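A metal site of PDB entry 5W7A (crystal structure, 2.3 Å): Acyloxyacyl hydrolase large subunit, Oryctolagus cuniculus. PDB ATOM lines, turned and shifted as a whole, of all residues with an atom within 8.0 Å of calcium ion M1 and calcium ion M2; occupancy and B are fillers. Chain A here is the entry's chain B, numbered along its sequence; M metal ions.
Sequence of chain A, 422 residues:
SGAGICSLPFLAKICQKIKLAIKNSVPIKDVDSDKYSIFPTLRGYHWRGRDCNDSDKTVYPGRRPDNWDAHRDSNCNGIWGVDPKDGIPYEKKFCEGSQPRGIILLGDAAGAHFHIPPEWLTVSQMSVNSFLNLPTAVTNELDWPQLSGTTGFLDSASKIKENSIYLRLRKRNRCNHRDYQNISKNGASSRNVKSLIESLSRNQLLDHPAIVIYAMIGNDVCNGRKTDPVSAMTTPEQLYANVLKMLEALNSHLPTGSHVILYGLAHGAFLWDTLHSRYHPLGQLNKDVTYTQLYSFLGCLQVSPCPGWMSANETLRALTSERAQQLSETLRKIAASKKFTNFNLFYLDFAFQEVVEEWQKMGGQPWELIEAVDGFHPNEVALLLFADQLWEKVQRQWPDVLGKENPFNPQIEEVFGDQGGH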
ATOM      1  N   PRO A  27      19.421 -30.510  24.339  1.00  0.00           N
ATOM      2  CA  PRO A  27      18.374 -31.349  23.752  1.00  0.00           C
ATOM      3  C   PRO A  27      18.336 -31.214  22.234  1.00  0.00           C
ATOM      4  O   PRO A  27      18.606 -30.157  21.670  1.00  0.00           O
ATOM      5  CB  PRO A  27      17.089 -30.824  24.391  1.00  0.00           C
ATOM      6  CG  PRO A  27      17.406 -29.419  24.779  1.00  0.00           C
ATOM      7  CD  PRO A  27      18.852 -29.434  25.180  1.00  0.00           C
ATOM      8  N   LYS A  29      15.403 -32.040  20.603  1.00  0.00           N
ATOM      9  CA  LYS A  29      14.059 -31.489  20.442  1.00  0.00           C
ATOM     10  C   LYS A  29      13.956 -30.219  21.271  1.00  0.00           C
ATOM     11  O   LYS A  29      13.836 -30.263  22.503  1.00  0.00           O
ATOM     12  CB  LYS A  29      13.028 -32.536  20.854  1.00  0.00           C
ATOM     13  CG  LYS A  29      11.564 -32.133  20.759  1.00  0.00           C
ATOM     14  CD  LYS A  29      11.211 -31.498  19.433  1.00  0.00           C
ATOM     15  CE  LYS A  29       9.730 -31.664  19.147  1.00  0.00           C
ATOM     16  NZ  LYS A  29       9.302 -30.878  17.971  1.00  0.00           N
ATOM     17  N   ASP A  30      14.017 -29.063  20.599  1.00  0.00           N
ATOM     18  CA  ASP A  30      14.077 -27.763  21.262  1.00  0.00           C
ATOM     19  C   ASP A  30      13.905 -26.655  20.234  1.00  0.00           C
ATOM     20  O   ASP A  30      14.894 -26.066  19.781  1.00  0.00           O
ATOM     21  CB  ASP A  30      15.423 -27.608  21.984  1.00  0.00           C
ATOM     22  CG  ASP A  30      15.532 -26.291  22.722  1.00  0.00           C
ATOM     23  OD1 ASP A  30      14.492 -25.644  22.959  1.00  0.00           O
ATOM     24  OD2 ASP A  30      16.667 -25.909  23.064  1.00  0.00           O
ATOM     25  N   VAL A  31      12.668 -26.361  19.837  1.00  0.00           N
ATOM     26  CA  VAL A  31      12.464 -25.506  18.682  1.00  0.00           C
ATOM     27  C   VAL A  31      12.983 -24.100  18.955  1.00  0.00           C
ATOM     28  O   VAL A  31      13.658 -23.499  18.111  1.00  0.00           O
ATOM     29  CB  VAL A  31      10.989 -25.492  18.257  1.00  0.00           C
ATOM     30  CG1 VAL A  31      10.793 -24.604  17.026  1.00  0.00           C
ATOM     31  CG2 VAL A  31      10.523 -26.907  17.961  1.00  0.00           C
ATOM     32  N   ASP A  32      12.694 -23.546  20.135  1.00  0.00           N
ATOM     33  CA  ASP A  32      13.119 -22.187  20.445  1.00  0.00           C
ATOM     34  C   ASP A  32      14.559 -22.121  20.939  1.00  0.00           C
ATOM     35  O   ASP A  32      15.041 -21.027  21.248  1.00  0.00           O
ATOM     36  CB  ASP A  32      12.187 -21.566  21.494  1.00  0.00           C
ATOM     37  CG  ASP A  32      12.085 -22.392  22.763  1.00  0.00           C
ATOM     38  OD1 ASP A  32      13.015 -23.162  23.036  1.00  0.00           O
ATOM     39  OD2 ASP A  32      11.076 -22.247  23.479  1.00  0.00           O
ATOM     40  N   SER A  33      15.255 -23.248  21.016  1.00  0.00           N
ATOM     41  CA  SER A  33      16.691 -23.262  21.345  1.00  0.00           C
ATOM     42  C   SER A  33      16.990 -22.563  22.662  1.00  0.00           C
ATOM     43  O   SER A  33      17.956 -21.797  22.764  1.00  0.00           O
ATOM     44  CB  SER A  33      17.507 -22.642  20.210  1.00  0.00           C
ATOM     45  OG  SER A  33      17.345 -23.371  19.006  1.00  0.00           O
ATOM     46  N   ASP A  34      16.174 -22.812  23.689  1.00  0.00           N
ATOM     47  CA  ASP A  34      16.475 -22.291  25.024  1.00  0.00           C
ATOM     48  C   ASP A  34      17.031 -23.367  25.946  1.00  0.00           C
ATOM     49  O   ASP A  34      17.265 -23.087  27.128  1.00  0.00           O
ATOM     50  CB  ASP A  34      15.222 -21.644  25.643  1.00  0.00           C
ATOM     51  CG  ASP A  34      14.071 -22.622  25.827  1.00  0.00           C
ATOM     52  OD1 ASP A  34      14.307 -23.853  25.798  1.00  0.00           O
ATOM     53  OD2 ASP A  34      12.940 -22.143  26.010  1.00  0.00           O
ATOM     54  N   LYS A  35      17.250 -24.577  25.442  1.00  0.00           N
ATOM     55  CA  LYS A  35      17.884 -25.732  26.100  1.00  0.00           C
ATOM     56  C   LYS A  35      16.893 -26.532  26.920  1.00  0.00           C
ATOM     57  O   LYS A  35      17.289 -27.498  27.582  1.00  0.00           O
ATOM     58  CB  LYS A  35      19.082 -25.346  26.998  1.00  0.00           C
ATOM     59  CG  LYS A  35      20.324 -25.096  26.188  1.00  0.00           C
ATOM     60  CD  LYS A  35      21.239 -24.091  26.837  1.00  0.00           C
ATOM     61  CE  LYS A  35      22.489 -23.902  26.010  1.00  0.00           C
ATOM     62  NZ  LYS A  35      23.171 -22.650  26.382  1.00  0.00           N
ATOM     63  N   TYR A  36      15.617 -26.172  26.901  1.00  0.00           N
ATOM     64  CA  TYR A  36      14.580 -26.934  27.588  1.00  0.00           C
ATOM     65  C   TYR A  36      13.656 -27.555  26.556  1.00  0.00           C
ATOM     66  O   TYR A  36      13.356 -26.940  25.528  1.00  0.00           O
ATOM     67  CB  TYR A  36      13.798 -26.020  28.539  1.00  0.00           C
ATOM     68  CG  TYR A  36      14.655 -25.495  29.666  1.00  0.00           C
ATOM     69  CD1 TYR A  36      14.824 -26.231  30.838  1.00  0.00           C
ATOM     70  CD2 TYR A  36      15.314 -24.279  29.570  1.00  0.00           C
ATOM     71  CE1 TYR A  36      15.607 -25.753  31.872  1.00  0.00           C
ATOM     72  CE2 TYR A  36      16.105 -23.798  30.602  1.00  0.00           C
ATOM     73  CZ  TYR A  36      16.247 -24.543  31.744  1.00  0.00           C
ATOM     74  OH  TYR A  36      17.022 -24.077  32.775  1.00  0.00           O
ATOM     75  N   SER A  37      13.221 -28.777  26.823  1.00  0.00           N
ATOM     76  CA  SER A  37      12.574 -29.603  25.820  1.00  0.00           C
ATOM     77  C   SER A  37      11.186 -30.017  26.283  1.00  0.00           C
ATOM     78  O   SER A  37      10.866 -29.954  27.487  1.00  0.00           O
ATOM     79  CB  SER A  37      13.429 -30.842  25.514  1.00  0.00           C
ATOM     80  OG  SER A  37      12.849 -31.660  24.518  1.00  0.00           O
ATOM     81  N   ILE A  38      10.350 -30.422  25.324  1.00  0.00           N
ATOM     82  CA  ILE A  38       9.119 -31.140  25.612  1.00  0.00           C
ATOM     83  C   ILE A  38       9.271 -32.639  25.411  1.00  0.00           C
ATOM     84  O   ILE A  38       8.299 -33.385  25.586  1.00  0.00           O
ATOM     85  CB  ILE A  38       7.939 -30.605  24.771  1.00  0.00           C
ATOM     86  CG1 ILE A  38       8.196 -30.855  23.276  1.00  0.00           C
ATOM     87  CG2 ILE A  38       7.735 -29.112  25.050  1.00  0.00           C
ATOM     88  CD1 ILE A  38       7.087 -30.384  22.354  1.00  0.00           C
ATOM     89  N   GLY A  49      14.161 -29.163  33.631  1.00  0.00           N
ATOM     90  CA  GLY A  49      12.739 -28.873  33.664  1.00  0.00           C
ATOM     91  C   GLY A  49      12.110 -28.813  32.290  1.00  0.00           C
ATOM     92  O   GLY A  49      12.707 -28.295  31.333  1.00  0.00           O
ATOM     93  N   ARG A  50      10.902 -29.340  32.174  1.00  0.00           N
ATOM     94  CA  ARG A  50      10.194 -29.344  30.897  1.00  0.00           C
ATOM     95  C   ARG A  50       9.809 -27.921  30.475  1.00  0.00           C
ATOM     96  O   ARG A  50       9.290 -27.141  31.286  1.00  0.00           O
ATOM     97  CB  ARG A  50       8.947 -30.213  30.993  1.00  0.00           C
ATOM     98  CG  ARG A  50       8.370 -30.575  29.640  1.00  0.00           C
ATOM     99  CD  ARG A  50       6.884 -30.899  29.717  1.00  0.00           C
ATOM    100  NE  ARG A  50       6.595 -32.069  30.548  1.00  0.00           N
ATOM    101  CZ  ARG A  50       6.278 -33.278  30.101  1.00  0.00           C
ATOM    102  NH1 ARG A  50       6.207 -33.522  28.796  1.00  0.00           N
ATOM    103  NH2 ARG A  50       6.032 -34.267  30.956  1.00  0.00           N
ATOM    104  N   ASP A  51      10.040 -27.611  29.203  1.00  0.00           N
ATOM    105  CA  ASP A  51       9.697 -26.316  28.624  1.00  0.00           C
ATOM    106  C   ASP A  51       8.189 -26.213  28.445  1.00  0.00           C
ATOM    107  O   ASP A  51       7.604 -26.909  27.606  1.00  0.00           O
ATOM    108  CB  ASP A  51      10.412 -26.158  27.283  1.00  0.00           C
ATOM    109  CG  ASP A  51      10.373 -24.736  26.770  1.00  0.00           C
ATOM    110  OD1 ASP A  51       9.637 -23.909  27.340  1.00  0.00           O
ATOM    111  OD2 ASP A  51      11.084 -24.452  25.785  1.00  0.00           O
ATOM    112  N   CYS A  52       7.545 -25.332  29.206  1.00  0.00           N
ATOM    113  CA  CYS A  52       6.099 -25.154  29.077  1.00  0.00           C
ATOM    114  C   CYS A  52       5.713 -24.357  27.831  1.00  0.00           C
ATOM    115  O   CYS A  52       4.517 -24.283  27.522  1.00  0.00           O
ATOM    116  CB  CYS A  52       5.532 -24.476  30.336  1.00  0.00           C
ATOM    117  SG  CYS A  52       6.241 -22.861  30.788  1.00  0.00           S
ATOM    118  N   ASN A  53       6.669 -23.782  27.100  1.00  0.00           N
ATOM    119  CA  ASN A  53       6.418 -23.200  25.773  1.00  0.00           C
ATOM    120  C   ASN A  53       7.703 -23.325  24.953  1.00  0.00           C
ATOM    121  O   ASN A  53       8.584 -22.462  25.020  1.00  0.00           O
ATOM    122  CB  ASN A  53       5.979 -21.741  25.864  1.00  0.00           C
ATOM    123  CG  ASN A  53       5.453 -21.202  24.535  1.00  0.00           C
ATOM    124  OD1 ASN A  53       5.864 -21.667  23.474  1.00  0.00           O
ATOM    125  ND2 ASN A  53       4.552 -20.216  24.591  1.00  0.00           N
ATOM    126  N   ASP A  54       7.808 -24.406  24.176  1.00  0.00           N
ATOM    127  CA  ASP A  54       8.982 -24.601  23.335  1.00  0.00           C
ATOM    128  C   ASP A  54       8.937 -23.783  22.053  1.00  0.00           C
ATOM    129  O   ASP A  54       9.730 -24.032  21.145  1.00  0.00           O
ATOM    130  CB  ASP A  54       9.156 -26.093  22.994  1.00  0.00           C
ATOM    131  CG  ASP A  54      10.533 -26.392  22.418  1.00  0.00           C
ATOM    132  OD1 ASP A  54      11.493 -25.688  22.787  1.00  0.00           O
ATOM    133  OD2 ASP A  54      10.651 -27.337  21.614  1.00  0.00           O
ATOM    134  N   SER A  55       8.018 -22.811  21.953  1.00  0.00           N
ATOM    135  CA  SER A  55       7.982 -21.862  20.853  1.00  0.00           C
ATOM    136  C   SER A  55       8.449 -20.478  21.260  1.00  0.00           C
ATOM    137  O   SER A  55       8.441 -19.574  20.416  1.00  0.00           O
ATOM    138  CB  SER A  55       6.563 -21.772  20.274  1.00  0.00           C
ATOM    139  OG  SER A  55       6.366 -22.722  19.239  1.00  0.00           O
ATOM    140  N   ASP A  56       8.839 -20.272  22.517  1.00  0.00           N
ATOM    141  CA  ASP A  56       9.200 -18.949  23.011  1.00  0.00           C
ATOM    142  C   ASP A  56      10.477 -19.063  23.838  1.00  0.00           C
ATOM    143  O   ASP A  56      10.491 -19.697  24.900  1.00  0.00           O
ATOM    144  CB  ASP A  56       8.066 -18.350  23.847  1.00  0.00           C
ATOM    145  CG  ASP A  56       8.259 -16.869  24.116  1.00  0.00           C
ATOM    146  OD1 ASP A  56       9.418 -16.409  24.087  1.00  0.00           O
ATOM    147  OD2 ASP A  56       7.245 -16.179  24.352  1.00  0.00           O
ATOM    148  N   LYS A  57      11.537 -18.429  23.346  1.00  0.00           N
ATOM    149  CA  LYS A  57      12.830 -18.437  24.035  1.00  0.00           C
ATOM    150  C   LYS A  57      12.787 -17.714  25.378  1.00  0.00           C
ATOM    151  O   LYS A  57      13.669 -17.926  26.211  1.00  0.00           O
ATOM    152  CB  LYS A  57      13.867 -17.797  23.102  1.00  0.00           C
ATOM    153  CG  LYS A  57      15.321 -17.943  23.495  1.00  0.00           C
ATOM    154  CD  LYS A  57      16.218 -17.350  22.401  1.00  0.00           C
ATOM    155  CE  LYS A  57      17.595 -16.955  22.929  1.00  0.00           C
ATOM    156  NZ  LYS A  57      18.534 -18.111  23.059  1.00  0.00           N
ATOM    157  N   THR A  58      11.777 -16.872  25.615  1.00  0.00           N
ATOM    158  CA  THR A  58      11.647 -16.139  26.869  1.00  0.00           C
ATOM    159  C   THR A  58      10.751 -16.845  27.878  1.00  0.00           C
ATOM    160  O   THR A  58      10.383 -16.248  28.893  1.00  0.00           O
ATOM    161  CB  THR A  58      11.092 -14.726  26.616  1.00  0.00           C
ATOM    162  OG1 THR A  58       9.754 -14.814  26.128  1.00  0.00           O
ATOM    163  CG2 THR A  58      11.948 -13.985  25.600  1.00  0.00           C
ATOM    164  N   VAL A  59      10.397 -18.101  27.618  1.00  0.00           N
ATOM    165  CA  VAL A  59       9.614 -18.914  28.548  1.00  0.00           C
ATOM    166  C   VAL A  59      10.430 -20.173  28.801  1.00  0.00           C
ATOM    167  O   VAL A  59      10.664 -20.969  27.881  1.00  0.00           O
ATOM    168  CB  VAL A  59       8.225 -19.257  27.981  1.00  0.00           C
ATOM    169  CG1 VAL A  59       7.459 -20.168  28.945  1.00  0.00           C
ATOM    170  CG2 VAL A  59       7.430 -18.006  27.711  1.00  0.00           C
ATOM    171  N   TYR A  60      10.875 -20.346  30.038  1.00  0.00           N
ATOM    172  CA  TYR A  60      11.707 -21.488  30.395  1.00  0.00           C
ATOM    173  C   TYR A  60      11.818 -21.526  31.919  1.00  0.00           C
ATOM    174  O   TYR A  60      11.630 -20.516  32.581  1.00  0.00           O
ATOM    175  CB  TYR A  60      13.102 -21.393  29.767  1.00  0.00           C
ATOM    176  CG  TYR A  60      13.810 -20.101  30.058  1.00  0.00           C
ATOM    177  CD1 TYR A  60      14.507 -19.927  31.239  1.00  0.00           C
ATOM    178  CD2 TYR A  60      13.753 -19.040  29.159  1.00  0.00           C
ATOM    179  CE1 TYR A  60      15.151 -18.729  31.521  1.00  0.00           C
ATOM    180  CE2 TYR A  60      14.398 -17.849  29.434  1.00  0.00           C
ATOM    181  CZ  TYR A  60      15.094 -17.700  30.613  1.00  0.00           C
ATOM    182  OH  TYR A  60      15.726 -16.509  30.884  1.00  0.00           O
ATOM    183  N   PRO A  61      12.159 -22.688  32.490  1.00  0.00           N
ATOM    184  CA  PRO A  61      12.261 -22.778  33.947  1.00  0.00           C
ATOM    185  C   PRO A  61      13.418 -21.942  34.483  1.00  0.00           C
ATOM    186  O   PRO A  61      14.468 -21.804  33.856  1.00  0.00           O
ATOM    187  CB  PRO A  61      12.500 -24.268  34.200  1.00  0.00           C
ATOM    188  CG  PRO A  61      12.100 -24.961  32.931  1.00  0.00           C
ATOM    189  CD  PRO A  61      12.418 -23.986  31.843  1.00  0.00           C
ATOM    190  N   SER A  74       5.715 -17.714  32.535  1.00  0.00           N
ATOM    191  CA  SER A  74       6.949 -17.516  31.776  1.00  0.00           C
ATOM    192  C   SER A  74       8.150 -18.258  32.357  1.00  0.00           C
ATOM    193  O   SER A  74       9.161 -18.392  31.661  1.00  0.00           O
ATOM    194  CB  SER A  74       7.281 -16.025  31.697  1.00  0.00           C
ATOM    195  OG  SER A  74       7.673 -15.525  32.967  1.00  0.00           O
ATOM    196  N   CYS A  76       7.600 -21.367  33.993  1.00  0.00           N
ATOM    197  CA  CYS A  76       7.203 -22.772  33.940  1.00  0.00           C
ATOM    198  C   CYS A  76       7.050 -23.426  35.320  1.00  0.00           C
ATOM    199  O   CYS A  76       7.066 -24.654  35.431  1.00  0.00           O
ATOM    200  CB  CYS A  76       8.190 -23.592  33.088  1.00  0.00           C
ATOM    201  SG  CYS A  76       8.195 -23.221  31.301  1.00  0.00           S
HETATM  202 CA    CA M   1      10.704 -22.024  25.795  1.00  0.00          CA
HETATM  203 CA    CA M   2      12.870 -25.056  24.405  1.00  0.00          CA
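Seven residues have an atom within 4 Å of calcium ion M1: Asp 32, Asp 34, Asp 51, Asn 53, Asp 54, Asp 56 and Val 59. The nearest printed residue that does not touch calcium ion M1 is Lys 57 (4.4 Å).
The side-chain carboxylate (OD1) of Asp 56 sits at hydrogen-bond distance from the side-chain hydroxyl (OG1) of Thr 58 (2.6 Å). OD2 of Asp 32 sits close to N of Ser 55 (3.5 Å). The backbone NH of Asp 56 lies within hydrogen-bond range of the side-chain amide oxygen of Asn 53, at 3.4 Å. The side-chain carboxylate (OD2) of Asp 30 sits at hydrogen-bond distance from the backbone NH (N) of Lys 35. The backbone NH (N) of Ser 55 sits at hydrogen-bond distance from the side-chain amide oxygen (OD1) of Asn 53, 2.9 Å away. The side-chain sulfur (SG) of Cys 52 forms a disulfide with the side-chain sulfur (SG) of Cys 76, at 2.1 Å. The backbone NH of Ser 33 lies close to the side-chain carboxylate of Asp 30 (3.2 Å). N of Asp 51 is in hydrogen-bond range of O of Ser 37, 3.0 Å away.
Of the 26 residues printed, 6 come within 4 Å of calcium ion M2. The nearest printed residue that does not touch calcium ion M2 is Ser 37 (4.5 Å).
OD2 of Asp 34 is bound to calcium ion M1, 2.2 Å away. The backbone carbonyl oxygen (O) of Asn 53 binds calcium ion M1 (2.3 Å). Calcium ion M1 is bound by the backbone carbonyl oxygen (O) of Val 59, at 2.3 Å. The side-chain carboxylate (OD2) of Asp 32 is bound to calcium ion M1 (2.4 Å). OD2 of Asp 51 is bound to calcium ion M1 (2.5 Å). O of Asp 56 binds calcium ion M1, at 2.5 Å. The side-chain carboxylate (OD1) of Asp 51 is bound to calcium ion M1.
Calcium ion M2 is bound by OD1 of Asp 54 (2.2 Å), O of Tyr 36 (2.2 Å), OD1 of Asp 30 (2.3 Å), OD1 of Asp 34 (2.3 Å), OD2 of Asp 51 (2.3 Å) and OD1 of Asp 32 (2.3 Å). Calcium ion M2 has six donor atoms within binding distance.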
